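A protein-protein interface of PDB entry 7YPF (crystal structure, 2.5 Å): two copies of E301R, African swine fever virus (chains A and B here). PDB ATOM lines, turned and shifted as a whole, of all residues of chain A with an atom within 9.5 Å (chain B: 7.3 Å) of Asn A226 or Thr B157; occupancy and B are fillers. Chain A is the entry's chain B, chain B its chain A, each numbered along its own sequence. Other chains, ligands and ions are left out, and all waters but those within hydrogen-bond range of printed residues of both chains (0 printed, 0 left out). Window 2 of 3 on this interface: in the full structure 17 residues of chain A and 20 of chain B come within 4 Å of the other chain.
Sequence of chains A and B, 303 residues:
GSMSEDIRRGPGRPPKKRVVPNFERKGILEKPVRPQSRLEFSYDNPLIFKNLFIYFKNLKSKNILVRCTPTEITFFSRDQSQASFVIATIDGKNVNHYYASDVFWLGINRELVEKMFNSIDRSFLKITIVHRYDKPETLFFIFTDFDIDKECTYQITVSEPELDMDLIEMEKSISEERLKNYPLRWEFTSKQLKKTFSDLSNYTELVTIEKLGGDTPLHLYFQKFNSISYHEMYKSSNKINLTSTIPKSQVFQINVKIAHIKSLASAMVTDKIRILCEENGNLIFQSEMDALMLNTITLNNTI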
ATOM      1  N   GLN A 223       4.318 -31.161  -3.398  1.00  0.00           N
ATOM      2  CA  GLN A 223       4.009 -29.737  -3.454  1.00  0.00           C
ATOM      3  C   GLN A 223       2.510 -29.530  -3.308  1.00  0.00           C
ATOM      4  O   GLN A 223       1.731 -30.006  -4.142  1.00  0.00           O
ATOM      5  CB  GLN A 223       4.507 -29.119  -4.763  1.00  0.00           C
ATOM      6  CG  GLN A 223       6.015 -28.975  -4.846  1.00  0.00           C
ATOM      7  CD  GLN A 223       6.439 -27.893  -5.817  1.00  0.00           C
ATOM      8  OE1 GLN A 223       6.746 -28.169  -6.976  1.00  0.00           O
ATOM      9  NE2 GLN A 223       6.457 -26.649  -5.350  1.00  0.00           N
ATOM     10  N   LYS A 224       2.111 -28.831  -2.250  1.00  0.00           N
ATOM     11  CA  LYS A 224       0.742 -28.361  -2.077  1.00  0.00           C
ATOM     12  C   LYS A 224       0.759 -26.838  -2.107  1.00  0.00           C
ATOM     13  O   LYS A 224       1.463 -26.204  -1.312  1.00  0.00           O
ATOM     14  CB  LYS A 224       0.140 -28.879  -0.771  1.00  0.00           C
ATOM     15  CG  LYS A 224       0.038 -30.393  -0.705  1.00  0.00           C
ATOM     16  CD  LYS A 224      -0.613 -30.858   0.587  1.00  0.00           C
ATOM     17  CE  LYS A 224      -1.566 -32.018   0.338  1.00  0.00           C
ATOM     18  NZ  LYS A 224      -0.838 -33.305   0.151  1.00  0.00           N
ATOM     19  N   PHE A 225      -0.008 -26.257  -3.026  1.00  0.00           N
ATOM     20  CA  PHE A 225       0.055 -24.822  -3.262  1.00  0.00           C
ATOM     21  C   PHE A 225      -0.618 -24.057  -2.129  1.00  0.00           C
ATOM     22  O   PHE A 225      -1.692 -24.438  -1.651  1.00  0.00           O
ATOM     23  CB  PHE A 225      -0.587 -24.489  -4.612  1.00  0.00           C
ATOM     24  CG  PHE A 225      -1.322 -23.179  -4.652  1.00  0.00           C
ATOM     25  CD1 PHE A 225      -0.637 -21.985  -4.813  1.00  0.00           C
ATOM     26  CD2 PHE A 225      -2.706 -23.145  -4.567  1.00  0.00           C
ATOM     27  CE1 PHE A 225      -1.316 -20.779  -4.865  1.00  0.00           C
ATOM     28  CE2 PHE A 225      -3.389 -21.945  -4.617  1.00  0.00           C
ATOM     29  CZ  PHE A 225      -2.694 -20.760  -4.766  1.00  0.00           C
ATOM     30  N   ASN A 226       0.042 -22.987  -1.686  1.00  0.00           N
ATOM     31  CA  ASN A 226      -0.463 -22.067  -0.668  1.00  0.00           C
ATOM     32  C   ASN A 226      -0.668 -22.730   0.693  1.00  0.00           C
ATOM     33  O   ASN A 226      -1.377 -22.187   1.545  1.00  0.00           O
ATOM     34  CB  ASN A 226      -1.764 -21.395  -1.121  1.00  0.00           C
ATOM     35  CG  ASN A 226      -1.738 -19.893  -0.929  1.00  0.00           C
ATOM     36  OD1 ASN A 226      -0.714 -19.244  -1.150  1.00  0.00           O
ATOM     37  ND2 ASN A 226      -2.866 -19.330  -0.512  1.00  0.00           N
ATOM     38  N   SER A 227      -0.069 -23.896   0.933  1.00  0.00           N
ATOM     39  CA  SER A 227      -0.103 -24.467   2.274  1.00  0.00           C
ATOM     40  C   SER A 227       1.269 -24.977   2.699  1.00  0.00           C
ATOM     41  O   SER A 227       1.925 -24.364   3.547  1.00  0.00           O
ATOM     42  CB  SER A 227      -1.139 -25.591   2.357  1.00  0.00           C
ATOM     43  OG  SER A 227      -0.751 -26.708   1.580  1.00  0.00           O
ATOM     44  N   ILE A 228       1.723 -26.083   2.114  1.00  0.00           N
ATOM     45  CA  ILE A 228       2.985 -26.691   2.527  1.00  0.00           C
ATOM     46  C   ILE A 228       3.582 -27.458   1.358  1.00  0.00           C
ATOM     47  O   ILE A 228       2.900 -28.257   0.710  1.00  0.00           O
ATOM     48  CB  ILE A 228       2.808 -27.620   3.747  1.00  0.00           C
ATOM     49  CG1 ILE A 228       4.101 -28.394   4.015  1.00  0.00           C
ATOM     50  CG2 ILE A 228       1.633 -28.571   3.542  1.00  0.00           C
ATOM     51  CD1 ILE A 228       4.064 -29.233   5.271  1.00  0.00           C
ATOM     52  N   SER A 229       4.858 -27.206   1.089  1.00  0.00           N
ATOM     53  CA  SER A 229       5.666 -28.059   0.236  1.00  0.00           C
ATOM     54  C   SER A 229       6.806 -28.630   1.065  1.00  0.00           C
ATOM     55  O   SER A 229       7.285 -27.997   2.012  1.00  0.00           O
ATOM     56  CB  SER A 229       6.222 -27.294  -0.972  1.00  0.00           C
ATOM     57  OG  SER A 229       5.175 -26.756  -1.760  1.00  0.00           O
ATOM     58  N   GLY B 107       2.401 -14.452  10.588  1.00  0.00           N
ATOM     59  CA  GLY B 107       1.395 -15.317  11.192  1.00  0.00           C
ATOM     60  C   GLY B 107       1.548 -16.738  10.680  1.00  0.00           C
ATOM     61  O   GLY B 107       1.745 -16.953   9.481  1.00  0.00           O
ATOM     62  N   ILE B 108       1.447 -17.705  11.591  1.00  0.00           N
ATOM     63  CA  ILE B 108       1.561 -19.121  11.260  1.00  0.00           C
ATOM     64  C   ILE B 108       0.352 -19.855  11.817  1.00  0.00           C
ATOM     65  O   ILE B 108       0.013 -19.696  12.996  1.00  0.00           O
ATOM     66  CB  ILE B 108       2.859 -19.743  11.813  1.00  0.00           C
ATOM     67  CG1 ILE B 108       4.088 -18.978  11.322  1.00  0.00           C
ATOM     68  CG2 ILE B 108       2.960 -21.212  11.422  1.00  0.00           C
ATOM     69  CD1 ILE B 108       5.388 -19.486  11.919  1.00  0.00           C
ATOM     70  N   ASN B 109      -0.294 -20.656  10.974  1.00  0.00           N
ATOM     71  CA  ASN B 109      -1.362 -21.546  11.413  1.00  0.00           C
ATOM     72  C   ASN B 109      -0.748 -22.759  12.103  1.00  0.00           C
ATOM     73  O   ASN B 109       0.008 -23.515  11.480  1.00  0.00           O
ATOM     74  CB  ASN B 109      -2.223 -21.966  10.221  1.00  0.00           C
ATOM     75  CG  ASN B 109      -3.278 -22.989  10.593  1.00  0.00           C
ATOM     76  OD1 ASN B 109      -2.987 -24.176  10.735  1.00  0.00           O
ATOM     77  ND2 ASN B 109      -4.517 -22.533  10.746  1.00  0.00           N
ATOM     78  N   LEU B 112      -1.236 -26.247  10.620  1.00  0.00           N
ATOM     79  CA  LEU B 112      -0.466 -26.505   9.407  1.00  0.00           C
ATOM     80  C   LEU B 112       0.910 -27.080   9.725  1.00  0.00           C
ATOM     81  O   LEU B 112       1.385 -27.991   9.037  1.00  0.00           O
ATOM     82  CB  LEU B 112      -0.336 -25.212   8.601  1.00  0.00           C
ATOM     83  CG  LEU B 112       0.437 -25.252   7.283  1.00  0.00           C
ATOM     84  CD1 LEU B 112      -0.166 -26.272   6.326  1.00  0.00           C
ATOM     85  CD2 LEU B 112       0.470 -23.869   6.650  1.00  0.00           C
ATOM     86  N   VAL B 113       1.567 -26.565  10.769  1.00  0.00           N
ATOM     87  CA  VAL B 113       2.940 -26.947  11.083  1.00  0.00           C
ATOM     88  C   VAL B 113       3.025 -27.961  12.214  1.00  0.00           C
ATOM     89  O   VAL B 113       4.137 -28.302  12.641  1.00  0.00           O
ATOM     90  CB  VAL B 113       3.791 -25.709  11.428  1.00  0.00           C
ATOM     91  CG1 VAL B 113       3.829 -24.746  10.252  1.00  0.00           C
ATOM     92  CG2 VAL B 113       3.248 -25.024  12.678  1.00  0.00           C
ATOM     93  N   GLU B 137       5.484 -14.673   1.269  1.00  0.00           N
ATOM     94  CA  GLU B 137       4.477 -15.382   2.009  1.00  0.00           C
ATOM     95  C   GLU B 137       4.971 -16.762   2.377  1.00  0.00           C
ATOM     96  O   GLU B 137       4.218 -17.637   2.625  1.00  0.00           O
ATOM     97  CB  GLU B 137       3.191 -15.460   1.218  1.00  0.00           C
ATOM     98  CG  GLU B 137       2.479 -14.133   1.086  1.00  0.00           C
ATOM     99  CD  GLU B 137       1.658 -14.053  -0.169  1.00  0.00           C
ATOM    100  OE1 GLU B 137       1.552 -15.055  -0.875  1.00  0.00           O
ATOM    101  OE2 GLU B 137       1.121 -12.989  -0.453  1.00  0.00           O
ATOM    102  N   THR B 138       6.267 -16.923   2.452  1.00  0.00           N
ATOM    103  CA  THR B 138       6.826 -18.202   2.747  1.00  0.00           C
ATOM    104  C   THR B 138       7.821 -18.232   3.860  1.00  0.00           C
ATOM    105  O   THR B 138       8.584 -17.358   4.019  1.00  0.00           O
ATOM    106  CB  THR B 138       7.508 -18.785   1.510  1.00  0.00           C
ATOM    107  OG1 THR B 138       6.528 -19.118   0.560  1.00  0.00           O
ATOM    108  CG2 THR B 138       8.211 -20.009   1.851  1.00  0.00           C
ATOM    109  N   LEU B 139       7.761 -19.268   4.657  1.00  0.00           N
ATOM    110  CA  LEU B 139       8.750 -19.480   5.705  1.00  0.00           C
ATOM    111  C   LEU B 139       9.378 -20.852   5.511  1.00  0.00           C
ATOM    112  O   LEU B 139       8.664 -21.855   5.400  1.00  0.00           O
ATOM    113  CB  LEU B 139       8.113 -19.370   7.095  1.00  0.00           C
ATOM    114  CG  LEU B 139       9.046 -19.136   8.285  1.00  0.00           C
ATOM    115  CD1 LEU B 139      10.020 -18.003   8.000  1.00  0.00           C
ATOM    116  CD2 LEU B 139       8.240 -18.846   9.544  1.00  0.00           C
ATOM    117  N   PHE B 141      11.687 -24.004   6.775  1.00  0.00           N
ATOM    118  CA  PHE B 141      12.232 -24.754   7.902  1.00  0.00           C
ATOM    119  C   PHE B 141      13.059 -25.903   7.347  1.00  0.00           C
ATOM    120  O   PHE B 141      12.523 -26.782   6.663  1.00  0.00           O
ATOM    121  CB  PHE B 141      11.123 -25.287   8.814  1.00  0.00           C
ATOM    122  CG  PHE B 141      10.266 -24.216   9.428  1.00  0.00           C
ATOM    123  CD1 PHE B 141       9.174 -23.706   8.746  1.00  0.00           C
ATOM    124  CD2 PHE B 141      10.544 -23.729  10.697  1.00  0.00           C
ATOM    125  CE1 PHE B 141       8.378 -22.721   9.311  1.00  0.00           C
ATOM    126  CE2 PHE B 141       9.752 -22.744  11.268  1.00  0.00           C
ATOM    127  CZ  PHE B 141       8.668 -22.241  10.573  1.00  0.00           C
ATOM    128  N   TYR B 154      11.027 -27.625   4.590  1.00  0.00           N
ATOM    129  CA  TYR B 154       9.602 -27.332   4.600  1.00  0.00           C
ATOM    130  C   TYR B 154       9.385 -25.918   4.081  1.00  0.00           C
ATOM    131  O   TYR B 154      10.022 -24.974   4.558  1.00  0.00           O
ATOM    132  CB  TYR B 154       9.018 -27.461   6.008  1.00  0.00           C
ATOM    133  CG  TYR B 154       8.918 -28.876   6.527  1.00  0.00           C
ATOM    134  CD1 TYR B 154      10.031 -29.530   7.034  1.00  0.00           C
ATOM    135  CD2 TYR B 154       7.704 -29.550   6.524  1.00  0.00           C
ATOM    136  CE1 TYR B 154       9.942 -30.821   7.515  1.00  0.00           C
ATOM    137  CE2 TYR B 154       7.605 -30.844   7.002  1.00  0.00           C
ATOM    138  CZ  TYR B 154       8.728 -31.474   7.496  1.00  0.00           C
ATOM    139  OH  TYR B 154       8.634 -32.760   7.974  1.00  0.00           O
ATOM    140  N   GLN B 155       8.499 -25.780   3.100  1.00  0.00           N
ATOM    141  CA  GLN B 155       8.030 -24.478   2.640  1.00  0.00           C
ATOM    142  C   GLN B 155       6.645 -24.249   3.233  1.00  0.00           C
ATOM    143  O   GLN B 155       5.673 -24.892   2.822  1.00  0.00           O
ATOM    144  CB  GLN B 155       7.999 -24.416   1.115  1.00  0.00           C
ATOM    145  CG  GLN B 155       9.327 -24.750   0.461  1.00  0.00           C
ATOM    146  CD  GLN B 155       9.365 -24.375  -1.006  1.00  0.00           C
ATOM    147  OE1 GLN B 155       8.601 -23.525  -1.461  1.00  0.00           O
ATOM    148  NE2 GLN B 155      10.260 -25.008  -1.756  1.00  0.00           N
ATOM    149  N   ILE B 156       6.555 -23.338   4.198  1.00  0.00           N
ATOM    150  CA  ILE B 156       5.313 -23.067   4.913  1.00  0.00           C
ATOM    151  C   ILE B 156       4.765 -21.727   4.448  1.00  0.00           C
ATOM    152  O   ILE B 156       5.484 -20.721   4.440  1.00  0.00           O
ATOM    153  CB  ILE B 156       5.522 -23.071   6.437  1.00  0.00           C
ATOM    154  CG1 ILE B 156       6.147 -24.392   6.889  1.00  0.00           C
ATOM    155  CG2 ILE B 156       4.200 -22.833   7.153  1.00  0.00           C
ATOM    156  CD1 ILE B 156       5.236 -25.585   6.723  1.00  0.00           C
ATOM    157  N   THR B 157       3.492 -21.717   4.065  1.00  0.00           N
ATOM    158  CA  THR B 157       2.815 -20.480   3.705  1.00  0.00           C
ATOM    159  C   THR B 157       2.400 -19.748   4.973  1.00  0.00           C
ATOM    160  O   THR B 157       1.713 -20.314   5.829  1.00  0.00           O
ATOM    161  CB  THR B 157       1.595 -20.768   2.832  1.00  0.00           C
ATOM    162  OG1 THR B 157       2.001 -21.471   1.652  1.00  0.00           O
ATOM    163  CG2 THR B 157       0.906 -19.472   2.432  1.00  0.00           C
ATOM    164  N   VAL B 158       2.825 -18.494   5.101  1.00  0.00           N
ATOM    165  CA  VAL B 158       2.525 -17.692   6.279  1.00  0.00           C
ATOM    166  C   VAL B 158       1.706 -16.477   5.866  1.00  0.00           C
ATOM    167  O   VAL B 158       1.809 -15.982   4.738  1.00  0.00           O
ATOM    168  CB  VAL B 158       3.810 -17.263   7.019  1.00  0.00           C
ATOM    169  CG1 VAL B 158       4.569 -18.487   7.502  1.00  0.00           C
ATOM    170  CG2 VAL B 158       4.688 -16.407   6.117  1.00  0.00           C
ATOM    171  N   SER B 159       0.876 -16.009   6.790  1.00  0.00           N
ATOM    172  CA  SER B 159       0.060 -14.819   6.605  1.00  0.00           C
ATOM    173  C   SER B 159       0.731 -13.598   7.226  1.00  0.00           C
ATOM    174  O   SER B 159       1.679 -13.704   8.008  1.00  0.00           O
ATOM    175  CB  SER B 159      -1.327 -15.024   7.219  1.00  0.00           C
ATOM    176  OG  SER B 159      -1.381 -16.240   7.946  1.00  0.00           O
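O of Phe B141 is in hydrogen-bond range of N of Tyr B154, 2.7 Å away.
OD1 of Asn B109 sits at hydrogen-bond distance from N of Leu B112 (2.7 Å).
N of Leu B139 sits at hydrogen-bond distance from O of Ile B156 (2.7 Å).
Hydrophobic or aromatic side chains of chain B that line the printed part of chain A: Leu B112 and Tyr B154.
Among the printed residues, 9 pairs touch across the chains.
Among the printed residues, no Asp or Glu carboxylate lies within 4 Å of a Lys or Arg side-chain nitrogen of the other chain.
The backbone carbonyl oxygen of Asn A226 sits close to the side-chain hydroxyl of Thr B157 (3.5 Å).
The backbone carbonyl oxygen (O) of Ser A229 lies within hydrogen-bond range of the backbone NH (N) of Gln B155, 2.8 Å away.
O of Ser A227 sits at hydrogen-bond distance from N of Thr B157.
Printed residues of chain B within 4 Å of Ile A228: Tyr B154 (3.9 Å) and Gln B155 (3.2 Å).
Of the printed residues of chain B, Ser A229 touches Tyr B154 (3.5 Å) and Gln B155 (2.8 Å).
Of the printed residues of chain A, Leu B112 touches Ser A227 (3.5 Å).
Of the printed residues of chain A, Gln B155 touches Ser A227, Ile A228 and Ser A229.
Ile B156 touches just one residue of chain A: Ser A227 (3.9 Å).
No residue of chain A comes within 4 Å of Val B158.
The nearest residue of chain B that does not touch Asn A226 is Glu B137 (4.8 Å).
No position is printed for both chains.
Of the 9 pairs that touch across the chains among the printed residues, none has its exchanged pair printed and touching as well.
Among the printed residues, pairs that only touch across the chains: Ile A228 with Gln B155, Ser A227 with Leu B112, Ser A229 with Tyr B154, Ser A227 with Gln B155, Ile A228 with Tyr B154 and Ser A227 with Ile B156.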
